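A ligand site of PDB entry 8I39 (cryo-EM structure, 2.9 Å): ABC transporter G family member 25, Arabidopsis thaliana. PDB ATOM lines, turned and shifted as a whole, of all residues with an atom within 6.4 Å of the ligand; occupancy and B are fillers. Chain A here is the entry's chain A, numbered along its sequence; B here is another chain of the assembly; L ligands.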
ATOM      1  N   GLN A 413     -32.872 -23.848  12.434  1.00  0.00           N
ATOM      2  CA  GLN A 413     -31.626 -23.108  12.332  1.00  0.00           C
ATOM      3  C   GLN A 413     -30.992 -23.231  10.953  1.00  0.00           C
ATOM      4  O   GLN A 413     -29.987 -22.571  10.695  1.00  0.00           O
ATOM      5  CB  GLN A 413     -30.646 -23.601  13.386  1.00  0.00           C
ATOM      6  CG  GLN A 413     -29.440 -22.752  13.551  1.00  0.00           C
ATOM      7  CD  GLN A 413     -28.565 -23.232  14.657  1.00  0.00           C
ATOM      8  OE1 GLN A 413     -28.948 -24.116  15.419  1.00  0.00           O
ATOM      9  NE2 GLN A 413     -27.381 -22.664  14.773  1.00  0.00           N
ATOM     10  N   ALA A 417     -31.205 -19.924   8.160  1.00  0.00           N
ATOM     11  CA  ALA A 417     -30.017 -19.507   7.432  1.00  0.00           C
ATOM     12  C   ALA A 417     -30.230 -19.560   5.932  1.00  0.00           C
ATOM     13  O   ALA A 417     -29.635 -18.759   5.202  1.00  0.00           O
ATOM     14  CB  ALA A 417     -28.829 -20.376   7.821  1.00  0.00           C
ATOM     15  N   PHE A 441     -17.945 -17.468   2.611  1.00  0.00           N
ATOM     16  CA  PHE A 441     -17.405 -17.592   3.944  1.00  0.00           C
ATOM     17  C   PHE A 441     -18.492 -17.682   4.998  1.00  0.00           C
ATOM     18  O   PHE A 441     -18.218 -18.146   6.101  1.00  0.00           O
ATOM     19  CB  PHE A 441     -16.499 -16.417   4.273  1.00  0.00           C
ATOM     20  CG  PHE A 441     -15.492 -16.719   5.331  1.00  0.00           C
ATOM     21  CD1 PHE A 441     -15.559 -16.103   6.556  1.00  0.00           C
ATOM     22  CD2 PHE A 441     -14.484 -17.611   5.109  1.00  0.00           C
ATOM     23  CE1 PHE A 441     -14.637 -16.380   7.518  1.00  0.00           C
ATOM     24  CE2 PHE A 441     -13.562 -17.888   6.071  1.00  0.00           C
ATOM     25  CZ  PHE A 441     -13.638 -17.272   7.276  1.00  0.00           C
ATOM     26  N   PHE A 442     -19.705 -17.243   4.704  1.00  0.00           N
ATOM     27  CA  PHE A 442     -20.812 -17.593   5.573  1.00  0.00           C
ATOM     28  C   PHE A 442     -21.178 -19.057   5.396  1.00  0.00           C
ATOM     29  O   PHE A 442     -21.330 -19.794   6.378  1.00  0.00           O
ATOM     30  CB  PHE A 442     -22.004 -16.703   5.313  1.00  0.00           C
ATOM     31  CG  PHE A 442     -23.255 -17.191   5.961  1.00  0.00           C
ATOM     32  CD1 PHE A 442     -24.317 -17.620   5.194  1.00  0.00           C
ATOM     33  CD2 PHE A 442     -23.361 -17.226   7.327  1.00  0.00           C
ATOM     34  CE1 PHE A 442     -25.468 -18.083   5.791  1.00  0.00           C
ATOM     35  CE2 PHE A 442     -24.505 -17.697   7.920  1.00  0.00           C
ATOM     36  CZ  PHE A 442     -25.556 -18.117   7.153  1.00  0.00           C
ATOM     37  N   ILE A 445     -18.555 -20.836   7.147  1.00  0.00           N
ATOM     38  CA  ILE A 445     -18.583 -20.691   8.593  1.00  0.00           C
ATOM     39  C   ILE A 445     -19.746 -21.466   9.177  1.00  0.00           C
ATOM     40  O   ILE A 445     -19.616 -22.121  10.211  1.00  0.00           O
ATOM     41  CB  ILE A 445     -18.685 -19.208   8.982  1.00  0.00           C
ATOM     42  CG1 ILE A 445     -17.320 -18.540   8.998  1.00  0.00           C
ATOM     43  CG2 ILE A 445     -19.314 -19.072  10.334  1.00  0.00           C
ATOM     44  CD1 ILE A 445     -17.412 -17.068   9.201  1.00  0.00           C
ATOM     45  N   PHE A 446     -20.909 -21.380   8.545  1.00  0.00           N
ATOM     46  CA  PHE A 446     -22.095 -22.040   9.057  1.00  0.00           C
ATOM     47  C   PHE A 446     -21.908 -23.538   9.138  1.00  0.00           C
ATOM     48  O   PHE A 446     -22.286 -24.164  10.131  1.00  0.00           O
ATOM     49  CB  PHE A 446     -23.284 -21.697   8.173  1.00  0.00           C
ATOM     50  CG  PHE A 446     -24.602 -22.062   8.774  1.00  0.00           C
ATOM     51  CD1 PHE A 446     -25.347 -23.086   8.263  1.00  0.00           C
ATOM     52  CD2 PHE A 446     -25.099 -21.350   9.844  1.00  0.00           C
ATOM     53  CE1 PHE A 446     -26.544 -23.407   8.811  1.00  0.00           C
ATOM     54  CE2 PHE A 446     -26.309 -21.678  10.379  1.00  0.00           C
ATOM     55  CZ  PHE A 446     -27.031 -22.707   9.863  1.00  0.00           C
ATOM     56  N   VAL A 449     -19.283 -25.000  11.831  1.00  0.00           N
ATOM     57  CA  VAL A 449     -19.700 -24.821  13.207  1.00  0.00           C
ATOM     58  C   VAL A 449     -20.932 -25.649  13.525  1.00  0.00           C
ATOM     59  O   VAL A 449     -21.044 -26.195  14.618  1.00  0.00           O
ATOM     60  CB  VAL A 449     -19.948 -23.321  13.489  1.00  0.00           C
ATOM     61  CG1 VAL A 449     -20.684 -23.165  14.784  1.00  0.00           C
ATOM     62  CG2 VAL A 449     -18.644 -22.575  13.522  1.00  0.00           C
ATOM     63  N   LEU A 450     -21.867 -25.754  12.590  1.00  0.00           N
ATOM     64  CA  LEU A 450     -23.068 -26.525  12.860  1.00  0.00           C
ATOM     65  C   LEU A 450     -22.756 -28.011  12.991  1.00  0.00           C
ATOM     66  O   LEU A 450     -23.256 -28.644  13.927  1.00  0.00           O
ATOM     67  CB  LEU A 450     -24.119 -26.248  11.799  1.00  0.00           C
ATOM     68  CG  LEU A 450     -25.552 -26.473  12.257  1.00  0.00           C
ATOM     69  CD1 LEU A 450     -25.916 -25.378  13.210  1.00  0.00           C
ATOM     70  CD2 LEU A 450     -26.514 -26.518  11.118  1.00  0.00           C
ATOM     71  N   VAL A 559     -11.973 -20.077  12.011  1.00  0.00           N
ATOM     72  CA  VAL A 559     -12.673 -19.058  11.252  1.00  0.00           C
ATOM     73  C   VAL A 559     -11.848 -17.796  11.115  1.00  0.00           C
ATOM     74  O   VAL A 559     -11.921 -17.109  10.096  1.00  0.00           O
ATOM     75  CB  VAL A 559     -14.032 -18.767  11.897  1.00  0.00           C
ATOM     76  CG1 VAL A 559     -14.539 -17.428  11.480  1.00  0.00           C
ATOM     77  CG2 VAL A 559     -15.029 -19.834  11.538  1.00  0.00           C
ATOM     78  N   TYR A 565     -11.155 -12.662   7.277  1.00  0.00           N
ATOM     79  CA  TYR A 565     -11.107 -11.478   8.120  1.00  0.00           C
ATOM     80  C   TYR A 565      -9.753 -10.782   8.026  1.00  0.00           C
ATOM     81  O   TYR A 565      -9.685  -9.550   7.975  1.00  0.00           O
ATOM     82  CB  TYR A 565     -11.426 -11.843   9.561  1.00  0.00           C
ATOM     83  CG  TYR A 565     -12.897 -12.068   9.800  1.00  0.00           C
ATOM     84  CD1 TYR A 565     -13.786 -11.027   9.775  1.00  0.00           C
ATOM     85  CD2 TYR A 565     -13.385 -13.336  10.030  1.00  0.00           C
ATOM     86  CE1 TYR A 565     -15.130 -11.225   9.978  1.00  0.00           C
ATOM     87  CE2 TYR A 565     -14.723 -13.541  10.231  1.00  0.00           C
ATOM     88  CZ  TYR A 565     -15.588 -12.494  10.210  1.00  0.00           C
ATOM     89  OH  TYR A 565     -16.930 -12.715  10.409  1.00  0.00           O
ATOM     90  N   PHE B 441     -15.425  -6.080  13.398  1.00  0.00           N
ATOM     91  CA  PHE B 441     -16.603  -6.909  13.209  1.00  0.00           C
ATOM     92  C   PHE B 441     -16.477  -8.260  13.873  1.00  0.00           C
ATOM     93  O   PHE B 441     -17.491  -8.910  14.120  1.00  0.00           O
ATOM     94  CB  PHE B 441     -16.893  -7.108  11.729  1.00  0.00           C
ATOM     95  CG  PHE B 441     -18.313  -7.437  11.429  1.00  0.00           C
ATOM     96  CD1 PHE B 441     -18.675  -8.668  10.954  1.00  0.00           C
ATOM     97  CD2 PHE B 441     -19.306  -6.511  11.632  1.00  0.00           C
ATOM     98  CE1 PHE B 441     -19.965  -8.960  10.686  1.00  0.00           C
ATOM     99  CE2 PHE B 441     -20.602  -6.807  11.357  1.00  0.00           C
ATOM    100  CZ  PHE B 441     -20.934  -8.029  10.892  1.00  0.00           C
ATOM    101  N   PHE B 442     -15.262  -8.712  14.172  1.00  0.00           N
ATOM    102  CA  PHE B 442     -15.143  -9.844  15.072  1.00  0.00           C
ATOM    103  C   PHE B 442     -15.443  -9.424  16.500  1.00  0.00           C
ATOM    104  O   PHE B 442     -16.218 -10.082  17.194  1.00  0.00           O
ATOM    105  CB  PHE B 442     -13.751 -10.446  14.975  1.00  0.00           C
ATOM    106  CG  PHE B 442     -13.456 -11.415  16.064  1.00  0.00           C
ATOM    107  CD1 PHE B 442     -12.488 -11.146  17.012  1.00  0.00           C
ATOM    108  CD2 PHE B 442     -14.169 -12.591  16.164  1.00  0.00           C
ATOM    109  CE1 PHE B 442     -12.230 -12.026  18.028  1.00  0.00           C
ATOM    110  CE2 PHE B 442     -13.904 -13.478  17.177  1.00  0.00           C
ATOM    111  CZ  PHE B 442     -12.938 -13.187  18.100  1.00  0.00           C
ATOM    112  N   ILE B 445     -19.049  -9.120  16.554  1.00  0.00           N
ATOM    113  CA  ILE B 445     -19.767 -10.384  16.450  1.00  0.00           C
ATOM    114  C   ILE B 445     -19.633 -11.166  17.748  1.00  0.00           C
ATOM    115  O   ILE B 445     -20.597 -11.766  18.219  1.00  0.00           O
ATOM    116  CB  ILE B 445     -19.245 -11.201  15.263  1.00  0.00           C
ATOM    117  CG1 ILE B 445     -19.902 -10.780  13.973  1.00  0.00           C
ATOM    118  CG2 ILE B 445     -19.494 -12.657  15.495  1.00  0.00           C
ATOM    119  CD1 ILE B 445     -19.284 -11.441  12.785  1.00  0.00           C
ATOM    120  N   VAL B 449     -23.032 -12.074  20.459  1.00  0.00           N
ATOM    121  CA  VAL B 449     -23.416 -13.474  20.538  1.00  0.00           C
ATOM    122  C   VAL B 449     -23.113 -14.060  21.907  1.00  0.00           C
ATOM    123  O   VAL B 449     -23.887 -14.854  22.433  1.00  0.00           O
ATOM    124  CB  VAL B 449     -22.730 -14.279  19.422  1.00  0.00           C
ATOM    125  CG1 VAL B 449     -22.866 -15.741  19.683  1.00  0.00           C
ATOM    126  CG2 VAL B 449     -23.313 -13.929  18.084  1.00  0.00           C
ATOM    127  N   VAL B 551     -32.494 -17.131  19.675  1.00  0.00           N
ATOM    128  CA  VAL B 551     -31.495 -16.084  19.891  1.00  0.00           C
ATOM    129  C   VAL B 551     -30.212 -16.380  19.144  1.00  0.00           C
ATOM    130  O   VAL B 551     -29.222 -15.672  19.313  1.00  0.00           O
ATOM    131  CB  VAL B 551     -31.170 -15.913  21.381  1.00  0.00           C
ATOM    132  CG1 VAL B 551     -30.268 -17.010  21.847  1.00  0.00           C
ATOM    133  CG2 VAL B 551     -30.559 -14.577  21.642  1.00  0.00           C
ATOM    134  N   THR B 552     -30.186 -17.443  18.342  1.00  0.00           N
ATOM    135  CA  THR B 552     -29.118 -17.714  17.401  1.00  0.00           C
ATOM    136  C   THR B 552     -29.547 -17.497  15.966  1.00  0.00           C
ATOM    137  O   THR B 552     -28.731 -17.130  15.135  1.00  0.00           O
ATOM    138  CB  THR B 552     -28.608 -19.142  17.560  1.00  0.00           C
ATOM    139  OG1 THR B 552     -28.101 -19.325  18.898  1.00  0.00           O
ATOM    140  CG2 THR B 552     -27.500 -19.415  16.610  1.00  0.00           C
ATOM    141  N   VAL B 553     -30.820 -17.724  15.676  1.00  0.00           N
ATOM    142  CA  VAL B 553     -31.400 -17.312  14.406  1.00  0.00           C
ATOM    143  C   VAL B 553     -31.618 -15.820  14.344  1.00  0.00           C
ATOM    144  O   VAL B 553     -31.813 -15.264  13.263  1.00  0.00           O
ATOM    145  CB  VAL B 553     -32.712 -18.089  14.200  1.00  0.00           C
ATOM    146  CG1 VAL B 553     -33.476 -17.589  13.003  1.00  0.00           C
ATOM    147  CG2 VAL B 553     -32.401 -19.547  14.044  1.00  0.00           C
ATOM    148  N   MET B 555     -29.383 -13.509  16.146  1.00  0.00           N
ATOM    149  CA  MET B 555     -28.036 -12.965  15.992  1.00  0.00           C
ATOM    150  C   MET B 555     -27.402 -13.357  14.670  1.00  0.00           C
ATOM    151  O   MET B 555     -26.300 -12.889  14.377  1.00  0.00           O
ATOM    152  CB  MET B 555     -27.145 -13.419  17.143  1.00  0.00           C
ATOM    153  CG  MET B 555     -27.456 -12.730  18.450  1.00  0.00           C
ATOM    154  SD  MET B 555     -27.459 -10.942  18.330  1.00  0.00           S
ATOM    155  CE  MET B 555     -25.789 -10.647  17.764  1.00  0.00           C
ATOM    156  N   LEU B 556     -28.043 -14.206  13.883  1.00  0.00           N
ATOM    157  CA  LEU B 556     -27.621 -14.442  12.519  1.00  0.00           C
ATOM    158  C   LEU B 556     -28.179 -13.377  11.593  1.00  0.00           C
ATOM    159  O   LEU B 556     -27.453 -12.839  10.757  1.00  0.00           O
ATOM    160  CB  LEU B 556     -28.080 -15.827  12.075  1.00  0.00           C
ATOM    161  CG  LEU B 556     -27.723 -16.369  10.703  1.00  0.00           C
ATOM    162  CD1 LEU B 556     -26.294 -16.809  10.677  1.00  0.00           C
ATOM    163  CD2 LEU B 556     -28.629 -17.522  10.392  1.00  0.00           C
ATOM    164  N   VAL B 559     -25.996 -10.348  12.341  1.00  0.00           N
ATOM    165  CA  VAL B 559     -24.625 -10.340  11.868  1.00  0.00           C
ATOM    166  C   VAL B 559     -24.560 -10.235  10.353  1.00  0.00           C
ATOM    167  O   VAL B 559     -23.626  -9.627   9.817  1.00  0.00           O
ATOM    168  CB  VAL B 559     -23.907 -11.600  12.365  1.00  0.00           C
ATOM    169  CG1 VAL B 559     -22.714 -11.888  11.519  1.00  0.00           C
ATOM    170  CG2 VAL B 559     -23.497 -11.431  13.801  1.00  0.00           C
ATOM    171  N   LEU B 560     -25.530 -10.794   9.642  1.00  0.00           N
ATOM    172  CA  LEU B 560     -25.540 -10.667   8.190  1.00  0.00           C
ATOM    173  C   LEU B 560     -25.853  -9.248   7.764  1.00  0.00           C
ATOM    174  O   LEU B 560     -25.192  -8.695   6.877  1.00  0.00           O
ATOM    175  CB  LEU B 560     -26.554 -11.635   7.581  1.00  0.00           C
ATOM    176  CG  LEU B 560     -26.256 -13.125   7.729  1.00  0.00           C
ATOM    177  CD1 LEU B 560     -27.244 -13.920   6.924  1.00  0.00           C
ATOM    178  CD2 LEU B 560     -24.852 -13.422   7.300  1.00  0.00           C
ATOM    179  N   TYR B 565     -20.586  -8.273   5.672  1.00  0.00           N
ATOM    180  CA  TYR B 565     -20.548  -9.319   4.653  1.00  0.00           C
ATOM    181  C   TYR B 565     -21.130  -8.823   3.338  1.00  0.00           C
ATOM    182  O   TYR B 565     -20.583  -9.129   2.267  1.00  0.00           O
ATOM    183  CB  TYR B 565     -21.285 -10.553   5.142  1.00  0.00           C
ATOM    184  CG  TYR B 565     -20.496 -11.364   6.137  1.00  0.00           C
ATOM    185  CD1 TYR B 565     -19.384 -12.074   5.742  1.00  0.00           C
ATOM    186  CD2 TYR B 565     -20.857 -11.406   7.457  1.00  0.00           C
ATOM    187  CE1 TYR B 565     -18.658 -12.800   6.647  1.00  0.00           C
ATOM    188  CE2 TYR B 565     -20.137 -12.125   8.365  1.00  0.00           C
ATOM    189  CZ  TYR B 565     -19.035 -12.826   7.959  1.00  0.00           C
ATOM    190  OH  TYR B 565     -18.319 -13.550   8.873  1.00  0.00           O
HETATM  191  C1  LIG L   1     -19.118 -15.422  12.395  1.00  0.00           C
HETATM  192  C2  LIG L   1     -20.283 -15.273  11.532  1.00  0.00           C
HETATM  193  C3  LIG L   1     -21.540 -15.744  11.754  1.00  0.00           C
HETATM  194  C4  LIG L   1     -22.019 -16.027  13.021  1.00  0.00           C
HETATM  195  C5  LIG L   1     -23.108 -16.723  13.245  1.00  0.00           C
HETATM  196  C6  LIG L   1     -22.430 -15.930  10.606  1.00  0.00           C
HETATM  197  C7  LIG L   1     -23.228 -17.896  14.163  1.00  0.00           C
HETATM  198  O1  LIG L   1     -22.174 -17.909  15.106  1.00  0.00           O
HETATM  199  C8  LIG L   1     -24.487 -17.523  14.875  1.00  0.00           C
HETATM  200  C9  LIG L   1     -25.632 -18.068  14.587  1.00  0.00           C
HETATM  201  C10 LIG L   1     -25.798 -19.150  13.624  1.00  0.00           C
HETATM  202  O2  LIG L   1     -26.859 -19.747  13.508  1.00  0.00           O
HETATM  203  C11 LIG L   1     -24.628 -19.477  12.747  1.00  0.00           C
HETATM  204  O3  LIG L   1     -19.190 -16.113  13.331  1.00  0.00           O
HETATM  205  C12 LIG L   1     -23.256 -19.244  13.406  1.00  0.00           C
HETATM  206  O4  LIG L   1     -18.145 -14.834  12.102  1.00  0.00           O
HETATM  207  C13 LIG L   1     -24.396 -16.400  15.845  1.00  0.00           C
HETATM  208  C14 LIG L   1     -22.976 -20.402  14.357  1.00  0.00           C
HETATM  209  C15 LIG L   1     -22.183 -19.296  12.324  1.00  0.00           C
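Merely in contact with the ligand: Phe 442 of chain A (3.6 Å), Ile 445 of chain A (3.5 Å), Phe 446 (3.5 Å), Val 449 of chain A (3.6 Å), Ile 445 of chain B (3.6 Å), Val 449 of chain B (3.5 Å), Thr 552 of chain B (3.1 Å) and Leu 556 of chain B (3.8 Å).
Hydrophobic or aromatic side chains within 4 Å of the ligand: Phe 442 of chain A, Ile 445 of chain A, Phe 446, Val 449 of chain A, Tyr 565 of chain A, Ile 445 of chain B, Val 449 of chain B and Leu 556 of chain B.
Of the 22 residues printed, 11 come within 4 Å of the ligand.
OH of Tyr 565 of chain B sits at hydrogen-bond distance from O4 of the ligand, at 3.5 Å.
The side-chain hydroxyl (OH) of Tyr 565 of chain A is in hydrogen-bond range of an oxygen (O4) of the ligand (3.0 Å).
NE2 of Gln 413 lies within hydrogen-bond range of O2 of the ligand (3.2 Å).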
